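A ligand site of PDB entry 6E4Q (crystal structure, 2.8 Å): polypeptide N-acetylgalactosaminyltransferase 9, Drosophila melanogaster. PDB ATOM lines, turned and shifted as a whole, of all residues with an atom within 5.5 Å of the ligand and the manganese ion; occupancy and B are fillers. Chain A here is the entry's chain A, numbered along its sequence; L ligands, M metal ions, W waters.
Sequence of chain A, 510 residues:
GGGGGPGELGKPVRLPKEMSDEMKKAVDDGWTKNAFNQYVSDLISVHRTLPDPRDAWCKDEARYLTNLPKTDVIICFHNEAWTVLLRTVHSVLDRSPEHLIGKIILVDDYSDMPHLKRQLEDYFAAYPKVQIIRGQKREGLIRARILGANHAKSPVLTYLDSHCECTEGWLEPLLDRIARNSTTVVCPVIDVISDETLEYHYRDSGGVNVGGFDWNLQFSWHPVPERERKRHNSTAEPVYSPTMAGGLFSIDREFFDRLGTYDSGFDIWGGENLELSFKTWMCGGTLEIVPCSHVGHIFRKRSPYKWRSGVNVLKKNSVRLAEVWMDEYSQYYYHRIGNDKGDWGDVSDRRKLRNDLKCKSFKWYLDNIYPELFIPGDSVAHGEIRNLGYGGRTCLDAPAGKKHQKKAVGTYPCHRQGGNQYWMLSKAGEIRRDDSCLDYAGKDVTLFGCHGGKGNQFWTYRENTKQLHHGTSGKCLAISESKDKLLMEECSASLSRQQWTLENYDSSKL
The manganese ion is bound by O7 of the ligand (2.1 Å), OD2 of Asp 161 (2.2 Å), O10 of the ligand (2.2 Å), NE2 of His 297 (2.3 Å), NE2 of His 163 (2.3 Å) and water W1 (2.6 Å).
Water W1 lies within hydrogen-bond range of NH1 of Arg 300 (2.9 Å), O11 of the ligand (3.3 Å) and O of Ile 298 (3.3 Å).
Merely in contact with the ligand: Phe 77 (3.1 Å), Gly 140 (3.7 Å) and Leu 141 (3.3 Å). Hydrophobic or aromatic side chains within 4 Å of the ligand: Phe 77, His 78, Leu 141, His 163, His 297 and Tyr 305. 13 residues have an atom within 4 Å of the ligand: Cys 76, Phe 77, His 78, Asp 109, Arg 138, Gly 140, Leu 141, Asp 161, Ser 162, His 163, His 297, Arg 300 and Tyr 305.
N of Ser 162 lies within hydrogen-bond range of O5 of the ligand, 2.7 Å away. OG of Ser 162 sits at hydrogen-bond distance from O5 of the ligand (2.7 Å). The guanidinium group (NE) of Arg 138 sits at hydrogen-bond distance from an oxygen (O2) of the ligand (2.8 Å). N2 of the ligand sits at hydrogen-bond distance from OD2 of Asp 109. O of Cys 76 is in hydrogen-bond range of O5 of the ligand, at 2.9 Å. The side-chain hydroxyl of Tyr 305 lies close to an oxygen (O8) of the ligand. The guanidinium group (NH1) of Arg 300 lies within salt-bridge range of an oxygen (O8) of the ligand, 3.3 Å away. The backbone NH (N) of His 78 sits at hydrogen-bond distance from an oxygen (O3) of the ligand.
A ring nitrogen (ND1) of His 163 lies within hydrogen-bond range of the side-chain carboxylate (OE1) of Glu 80, at 3.0 Å. The side-chain hydroxyl of Ser 162 is in hydrogen-bond range of the side-chain carboxylate of Glu 80 (2.7 Å). NE of Arg 138 is in salt-bridge range of OD2 of Asp 109. The guanidinium group of Arg 138 sits close to a ring nitrogen (NE2) of His 78. The side-chain carboxylate (OD2) of Asp 109 lies within hydrogen-bond range of the backbone NH (N) of Gly 140 (3.2 Å). N of Glu 139 sits at hydrogen-bond distance from OD1 of Asp 109, at 2.7 Å. The backbone NH of Arg 145 sits at hydrogen-bond distance from the side-chain sulfur of Cys 76. The side-chain hydroxyl (OH) of Tyr 305 sits at hydrogen-bond distance from the guanidinium group (NH2) of Arg 300, at 3.3 Å.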
ATOM      1  N   ILE A  75      22.381   5.175 -12.757  1.00  0.00           N
ATOM      2  CA  ILE A  75      22.263   6.353 -13.628  1.00  0.00           C
ATOM      3  C   ILE A  75      21.537   7.436 -12.833  1.00  0.00           C
ATOM      4  O   ILE A  75      20.306   7.411 -12.714  1.00  0.00           O
ATOM      5  CB  ILE A  75      21.507   6.022 -14.921  1.00  0.00           C
ATOM      6  CG1 ILE A  75      22.020   4.737 -15.557  1.00  0.00           C
ATOM      7  CG2 ILE A  75      21.600   7.189 -15.910  1.00  0.00           C
ATOM      8  CD1 ILE A  75      21.196   4.265 -16.753  1.00  0.00           C
ATOM      9  N   CYS A  76      22.257   8.428 -12.316  1.00  0.00           N
ATOM     10  CA  CYS A  76      21.529   9.553 -11.723  1.00  0.00           C
ATOM     11  C   CYS A  76      21.032  10.510 -12.812  1.00  0.00           C
ATOM     12  O   CYS A  76      21.583  10.555 -13.924  1.00  0.00           O
ATOM     13  CB  CYS A  76      22.387  10.312 -10.733  1.00  0.00           C
ATOM     14  SG  CYS A  76      23.101   9.306  -9.412  1.00  0.00           S
ATOM     15  N   PHE A  77      19.980  11.258 -12.497  1.00  0.00           N
ATOM     16  CA  PHE A  77      19.431  12.199 -13.475  1.00  0.00           C
ATOM     17  C   PHE A  77      18.657  13.304 -12.765  1.00  0.00           C
ATOM     18  O   PHE A  77      18.335  13.191 -11.584  1.00  0.00           O
ATOM     19  CB  PHE A  77      18.556  11.485 -14.517  1.00  0.00           C
ATOM     20  CG  PHE A  77      17.322  10.857 -13.950  1.00  0.00           C
ATOM     21  CD1 PHE A  77      17.368   9.586 -13.420  1.00  0.00           C
ATOM     22  CD2 PHE A  77      16.105  11.534 -13.982  1.00  0.00           C
ATOM     23  CE1 PHE A  77      16.218   9.002 -12.907  1.00  0.00           C
ATOM     24  CE2 PHE A  77      14.956  10.972 -13.470  1.00  0.00           C
ATOM     25  CZ  PHE A  77      15.009   9.697 -12.934  1.00  0.00           C
ATOM     26  N   HIS A  78      18.407  14.400 -13.478  1.00  0.00           N
ATOM     27  CA  HIS A  78      17.532  15.480 -13.012  1.00  0.00           C
ATOM     28  C   HIS A  78      16.981  16.202 -14.234  1.00  0.00           C
ATOM     29  O   HIS A  78      17.737  16.864 -14.948  1.00  0.00           O
ATOM     30  CB  HIS A  78      18.266  16.479 -12.116  1.00  0.00           C
ATOM     31  CG  HIS A  78      17.422  17.674 -11.758  1.00  0.00           C
ATOM     32  ND1 HIS A  78      16.686  17.762 -10.604  1.00  0.00           N
ATOM     33  CD2 HIS A  78      17.186  18.824 -12.441  1.00  0.00           C
ATOM     34  CE1 HIS A  78      16.039  18.904 -10.570  1.00  0.00           C
ATOM     35  NE2 HIS A  78      16.317  19.573 -11.676  1.00  0.00           N
ATOM     36  N   GLU A  80      16.168  14.974 -16.980  1.00  0.00           N
ATOM     37  CA  GLU A  80      16.713  14.441 -18.215  1.00  0.00           C
ATOM     38  C   GLU A  80      15.613  14.204 -19.255  1.00  0.00           C
ATOM     39  O   GLU A  80      14.456  13.941 -18.918  1.00  0.00           O
ATOM     40  CB  GLU A  80      17.472  13.137 -17.960  1.00  0.00           C
ATOM     41  CG  GLU A  80      18.153  12.601 -19.207  1.00  0.00           C
ATOM     42  CD  GLU A  80      19.077  13.629 -19.840  1.00  0.00           C
ATOM     43  OE1 GLU A  80      20.307  13.590 -19.585  1.00  0.00           O
ATOM     44  OE2 GLU A  80      18.565  14.504 -20.589  1.00  0.00           O
ATOM     45  N   ASP A 109      16.760  12.310  -7.918  1.00  0.00           N
ATOM     46  CA  ASP A 109      17.226  13.658  -7.485  1.00  0.00           C
ATOM     47  C   ASP A 109      16.216  14.773  -7.782  1.00  0.00           C
ATOM     48  O   ASP A 109      16.546  15.824  -8.361  1.00  0.00           O
ATOM     49  CB  ASP A 109      18.586  14.018  -8.077  1.00  0.00           C
ATOM     50  CG  ASP A 109      19.208  15.224  -7.375  1.00  0.00           C
ATOM     51  OD1 ASP A 109      18.875  15.411  -6.198  1.00  0.00           O
ATOM     52  OD2 ASP A 109      19.994  15.981  -7.988  1.00  0.00           O
ATOM     53  N   ARG A 138      16.264  18.010  -3.942  1.00  0.00           N
ATOM     54  CA  ARG A 138      17.423  18.117  -4.808  1.00  0.00           C
ATOM     55  C   ARG A 138      18.677  18.102  -3.948  1.00  0.00           C
ATOM     56  O   ARG A 138      18.829  18.900  -3.022  1.00  0.00           O
ATOM     57  CB  ARG A 138      17.359  19.377  -5.659  1.00  0.00           C
ATOM     58  CG  ARG A 138      18.511  19.609  -6.650  1.00  0.00           C
ATOM     59  CD  ARG A 138      18.339  18.905  -7.990  1.00  0.00           C
ATOM     60  NE  ARG A 138      19.205  19.543  -8.980  1.00  0.00           N
ATOM     61  CZ  ARG A 138      18.837  20.647  -9.643  1.00  0.00           C
ATOM     62  NH1 ARG A 138      19.645  21.237 -10.524  1.00  0.00           N
ATOM     63  NH2 ARG A 138      17.639  21.185  -9.393  1.00  0.00           N
ATOM     64  N   GLU A 139      19.563  17.162  -4.231  1.00  0.00           N
ATOM     65  CA  GLU A 139      20.742  16.992  -3.426  1.00  0.00           C
ATOM     66  C   GLU A 139      21.999  16.942  -4.260  1.00  0.00           C
ATOM     67  O   GLU A 139      23.099  16.948  -3.683  1.00  0.00           O
ATOM     68  CB  GLU A 139      20.654  15.695  -2.595  1.00  0.00           C
ATOM     69  CG  GLU A 139      19.607  15.734  -1.487  1.00  0.00           C
ATOM     70  CD  GLU A 139      20.222  15.852  -0.083  1.00  0.00           C
ATOM     71  OE1 GLU A 139      20.085  14.896   0.700  1.00  0.00           O
ATOM     72  OE2 GLU A 139      20.861  16.895   0.213  1.00  0.00           O
ATOM     73  N   GLY A 140      21.875  16.913  -5.578  1.00  0.00           N
ATOM     74  CA  GLY A 140      23.035  16.903  -6.435  1.00  0.00           C
ATOM     75  C   GLY A 140      23.550  15.507  -6.742  1.00  0.00           C
ATOM     76  O   GLY A 140      23.205  14.507  -6.116  1.00  0.00           O
ATOM     77  N   LEU A 141      24.444  15.481  -7.714  1.00  0.00           N
ATOM     78  CA  LEU A 141      25.022  14.241  -8.209  1.00  0.00           C
ATOM     79  C   LEU A 141      25.702  13.422  -7.110  1.00  0.00           C
ATOM     80  O   LEU A 141      25.453  12.212  -6.979  1.00  0.00           O
ATOM     81  CB  LEU A 141      26.005  14.617  -9.319  1.00  0.00           C
ATOM     82  CG  LEU A 141      27.030  13.636  -9.821  1.00  0.00           C
ATOM     83  CD1 LEU A 141      26.272  12.786 -10.855  1.00  0.00           C
ATOM     84  CD2 LEU A 141      28.235  14.373 -10.404  1.00  0.00           C
ATOM     85  N   ALA A 144      23.429  11.657  -4.716  1.00  0.00           N
ATOM     86  CA  ALA A 144      22.574  10.724  -5.433  1.00  0.00           C
ATOM     87  C   ALA A 144      23.298   9.429  -5.758  1.00  0.00           C
ATOM     88  O   ALA A 144      22.754   8.334  -5.588  1.00  0.00           O
ATOM     89  CB  ALA A 144      22.026  11.368  -6.709  1.00  0.00           C
ATOM     90  N   ARG A 145      24.532   9.530  -6.263  1.00  0.00           N
ATOM     91  CA  ARG A 145      25.290   8.308  -6.494  1.00  0.00           C
ATOM     92  C   ARG A 145      25.448   7.501  -5.203  1.00  0.00           C
ATOM     93  O   ARG A 145      25.461   6.257  -5.240  1.00  0.00           O
ATOM     94  CB  ARG A 145      26.668   8.613  -7.083  1.00  0.00           C
ATOM     95  CG  ARG A 145      26.743   9.197  -8.500  1.00  0.00           C
ATOM     96  CD  ARG A 145      28.233   9.308  -8.847  1.00  0.00           C
ATOM     97  NE  ARG A 145      28.626  10.376  -9.775  1.00  0.00           N
ATOM     98  CZ  ARG A 145      28.448  10.381 -11.085  1.00  0.00           C
ATOM     99  NH1 ARG A 145      27.831   9.394 -11.714  1.00  0.00           N
ATOM    100  NH2 ARG A 145      28.886  11.437 -11.783  1.00  0.00           N
ATOM    101  N   LEU A 160      26.787   5.672 -14.876  1.00  0.00           N
ATOM    102  CA  LEU A 160      26.659   6.279 -16.193  1.00  0.00           C
ATOM    103  C   LEU A 160      25.830   7.547 -16.053  1.00  0.00           C
ATOM    104  O   LEU A 160      24.866   7.570 -15.291  1.00  0.00           O
ATOM    105  CB  LEU A 160      25.984   5.322 -17.186  1.00  0.00           C
ATOM    106  CG  LEU A 160      26.630   3.977 -17.527  1.00  0.00           C
ATOM    107  CD1 LEU A 160      25.706   3.250 -18.479  1.00  0.00           C
ATOM    108  CD2 LEU A 160      27.987   4.121 -18.155  1.00  0.00           C
ATOM    109  N   ASP A 161      26.183   8.578 -16.810  1.00  0.00           N
ATOM    110  CA  ASP A 161      25.311   9.731 -16.938  1.00  0.00           C
ATOM    111  C   ASP A 161      24.015   9.345 -17.664  1.00  0.00           C
ATOM    112  O   ASP A 161      23.942   8.318 -18.332  1.00  0.00           O
ATOM    113  CB  ASP A 161      26.002  10.865 -17.695  1.00  0.00           C
ATOM    114  CG  ASP A 161      27.062  11.545 -16.851  1.00  0.00           C
ATOM    115  OD1 ASP A 161      27.462  10.954 -15.820  1.00  0.00           O
ATOM    116  OD2 ASP A 161      27.489  12.666 -17.217  1.00  0.00           O
ATOM    117  N   SER A 162      22.989  10.170 -17.521  1.00  0.00           N
ATOM    118  CA  SER A 162      21.717   9.880 -18.176  1.00  0.00           C
ATOM    119  C   SER A 162      21.731  10.182 -19.665  1.00  0.00           C
ATOM    120  O   SER A 162      20.708   9.994 -20.334  1.00  0.00           O
ATOM    121  CB  SER A 162      20.578  10.666 -17.507  1.00  0.00           C
ATOM    122  OG  SER A 162      20.902  12.023 -17.422  1.00  0.00           O
ATOM    123  N   HIS A 163      22.828  10.706 -20.199  1.00  0.00           N
ATOM    124  CA  HIS A 163      22.885  10.950 -21.629  1.00  0.00           C
ATOM    125  C   HIS A 163      24.067  10.195 -22.232  1.00  0.00           C
ATOM    126  O   HIS A 163      24.993  10.800 -22.771  1.00  0.00           O
ATOM    127  CB  HIS A 163      22.961  12.461 -21.904  1.00  0.00           C
ATOM    128  CG  HIS A 163      23.802  13.193 -20.913  1.00  0.00           C
ATOM    129  ND1 HIS A 163      23.333  13.588 -19.676  1.00  0.00           N
ATOM    130  CD2 HIS A 163      25.091  13.620 -20.982  1.00  0.00           C
ATOM    131  CE1 HIS A 163      24.302  14.199 -19.014  1.00  0.00           C
ATOM    132  NE2 HIS A 163      25.376  14.241 -19.789  1.00  0.00           N
ATOM    133  N   ILE A 268      27.463  20.548  -4.197  1.00  0.00           N
ATOM    134  CA  ILE A 268      27.204  20.085  -5.567  1.00  0.00           C
ATOM    135  C   ILE A 268      28.401  20.308  -6.513  1.00  0.00           C
ATOM    136  O   ILE A 268      28.719  19.447  -7.344  1.00  0.00           O
ATOM    137  CB  ILE A 268      25.924  20.744  -6.111  1.00  0.00           C
ATOM    138  CG1 ILE A 268      24.751  20.403  -5.188  1.00  0.00           C
ATOM    139  CG2 ILE A 268      25.679  20.344  -7.575  1.00  0.00           C
ATOM    140  CD1 ILE A 268      23.396  20.625  -5.792  1.00  0.00           C
ATOM    141  N   HIS A 297      28.819   9.704 -24.919  1.00  0.00           N
ATOM    142  CA  HIS A 297      28.284  10.682 -23.980  1.00  0.00           C
ATOM    143  C   HIS A 297      27.926  11.948 -24.758  1.00  0.00           C
ATOM    144  O   HIS A 297      28.632  12.312 -25.720  1.00  0.00           O
ATOM    145  CB  HIS A 297      29.286  10.977 -22.855  1.00  0.00           C
ATOM    146  CG  HIS A 297      28.961  12.179 -22.016  1.00  0.00           C
ATOM    147  ND1 HIS A 297      29.748  13.320 -22.015  1.00  0.00           N
ATOM    148  CD2 HIS A 297      27.980  12.413 -21.121  1.00  0.00           C
ATOM    149  CE1 HIS A 297      29.241  14.209 -21.173  1.00  0.00           C
ATOM    150  NE2 HIS A 297      28.169  13.679 -20.621  1.00  0.00           N
ATOM    151  N   ILE A 298      26.828  12.588 -24.383  1.00  0.00           N
ATOM    152  CA  ILE A 298      26.416  13.848 -25.002  1.00  0.00           C
ATOM    153  C   ILE A 298      27.141  14.986 -24.270  1.00  0.00           C
ATOM    154  O   ILE A 298      26.754  15.393 -23.184  1.00  0.00           O
ATOM    155  CB  ILE A 298      24.901  14.042 -24.953  1.00  0.00           C
ATOM    156  CG1 ILE A 298      24.193  12.908 -25.686  1.00  0.00           C
ATOM    157  CG2 ILE A 298      24.512  15.391 -25.562  1.00  0.00           C
ATOM    158  CD1 ILE A 298      22.746  13.211 -26.003  1.00  0.00           C
ATOM    159  N   ARG A 300      27.987  18.723 -23.466  1.00  0.00           N
ATOM    160  CA  ARG A 300      27.233  19.972 -23.516  1.00  0.00           C
ATOM    161  C   ARG A 300      28.171  21.158 -23.263  1.00  0.00           C
ATOM    162  O   ARG A 300      29.139  21.056 -22.514  1.00  0.00           O
ATOM    163  CB  ARG A 300      26.140  20.003 -22.465  1.00  0.00           C
ATOM    164  CG  ARG A 300      25.143  18.877 -22.456  1.00  0.00           C
ATOM    165  CD  ARG A 300      23.944  19.376 -21.662  1.00  0.00           C
ATOM    166  NE  ARG A 300      23.132  18.390 -20.953  1.00  0.00           N
ATOM    167  CZ  ARG A 300      23.405  17.924 -19.739  1.00  0.00           C
ATOM    168  NH1 ARG A 300      24.508  18.312 -19.114  1.00  0.00           N
ATOM    169  NH2 ARG A 300      22.577  17.050 -19.172  1.00  0.00           N
ATOM    170  N   SER A 303      25.775  23.601 -18.404  1.00  0.00           N
ATOM    171  CA  SER A 303      24.820  22.800 -17.625  1.00  0.00           C
ATOM    172  C   SER A 303      23.618  23.653 -17.228  1.00  0.00           C
ATOM    173  O   SER A 303      23.796  24.755 -16.688  1.00  0.00           O
ATOM    174  CB  SER A 303      25.475  22.235 -16.366  1.00  0.00           C
ATOM    175  OG  SER A 303      25.196  23.058 -15.245  1.00  0.00           O
ATOM    176  N   TYR A 305      21.439  23.695 -14.763  1.00  0.00           N
ATOM    177  CA  TYR A 305      21.021  23.333 -13.410  1.00  0.00           C
ATOM    178  C   TYR A 305      20.969  24.563 -12.514  1.00  0.00           C
ATOM    179  O   TYR A 305      21.705  25.530 -12.710  1.00  0.00           O
ATOM    180  CB  TYR A 305      21.979  22.303 -12.823  1.00  0.00           C
ATOM    181  CG  TYR A 305      22.062  21.048 -13.634  1.00  0.00           C
ATOM    182  CD1 TYR A 305      20.922  20.455 -14.148  1.00  0.00           C
ATOM    183  CD2 TYR A 305      23.297  20.449 -13.891  1.00  0.00           C
ATOM    184  CE1 TYR A 305      20.997  19.300 -14.898  1.00  0.00           C
ATOM    185  CE2 TYR A 305      23.385  19.290 -14.643  1.00  0.00           C
ATOM    186  CZ  TYR A 305      22.227  18.725 -15.147  1.00  0.00           C
ATOM    187  OH  TYR A 305      22.306  17.579 -15.895  1.00  0.00           O
HETATM  188  N1  LIG L   1      22.485  15.253 -12.337  1.00  0.00           N
HETATM  189  C1  LIG L   1      22.197  14.878 -11.037  1.00  0.00           C
HETATM  190  N2  LIG L   1      21.857  15.833 -10.094  1.00  0.00           N
HETATM  191  C2  LIG L   1      21.797  17.164 -10.441  1.00  0.00           C
HETATM  192  C3  LIG L   1      22.095  17.516 -11.756  1.00  0.00           C
HETATM  193  C4  LIG L   1      22.708  16.573 -12.580  1.00  0.00           C
HETATM  194  O1  LIG L   1      22.250  13.684 -10.729  1.00  0.00           O
HETATM  195  O2  LIG L   1      21.487  18.016  -9.591  1.00  0.00           O
HETATM  196  C5  LIG L   1      22.840  14.171 -13.298  1.00  0.00           C
HETATM  197  C6  LIG L   1      22.544  14.432 -14.772  1.00  0.00           C
HETATM  198  O3  LIG L   1      21.209  14.136 -15.163  1.00  0.00           O
HETATM  199  C7  LIG L   1      23.586  13.547 -15.453  1.00  0.00           C
HETATM  200  C8  LIG L   1      24.692  13.299 -14.435  1.00  0.00           C
HETATM  201  O4  LIG L   1      24.221  13.845 -13.211  1.00  0.00           O
HETATM  202  O5  LIG L   1      23.025  12.297 -15.789  1.00  0.00           O
HETATM  203  C9  LIG L   1      26.013  13.960 -14.807  1.00  0.00           C
HETATM  204  O6  LIG L   1      25.813  15.354 -14.841  1.00  0.00           O
HETATM  205  P1  LIG L   1      26.291  16.291 -16.069  1.00  0.00           P
HETATM  206  O7  LIG L   1      26.133  15.588 -17.350  1.00  0.00           O
HETATM  207  O8  LIG L   1      25.496  17.542 -16.099  1.00  0.00           O
HETATM  208  O9  LIG L   1      27.858  16.535 -15.803  1.00  0.00           O
HETATM  209  P2  LIG L   1      28.943  16.638 -17.005  1.00  0.00           P
HETATM  210  O10 LIG L   1      29.114  15.295 -17.636  1.00  0.00           O
HETATM  211  O11 LIG L   1      28.439  17.612 -18.014  1.00  0.00           O
HETATM  212  O12 LIG L   1      30.249  17.068 -16.423  1.00  0.00           O
HETATM  213 MN    MN M   1      27.328  14.370 -18.637  1.00  0.00          MN
HETATM  214  O   HOH W   1      26.256  16.256 -20.044  1.00  0.00           O
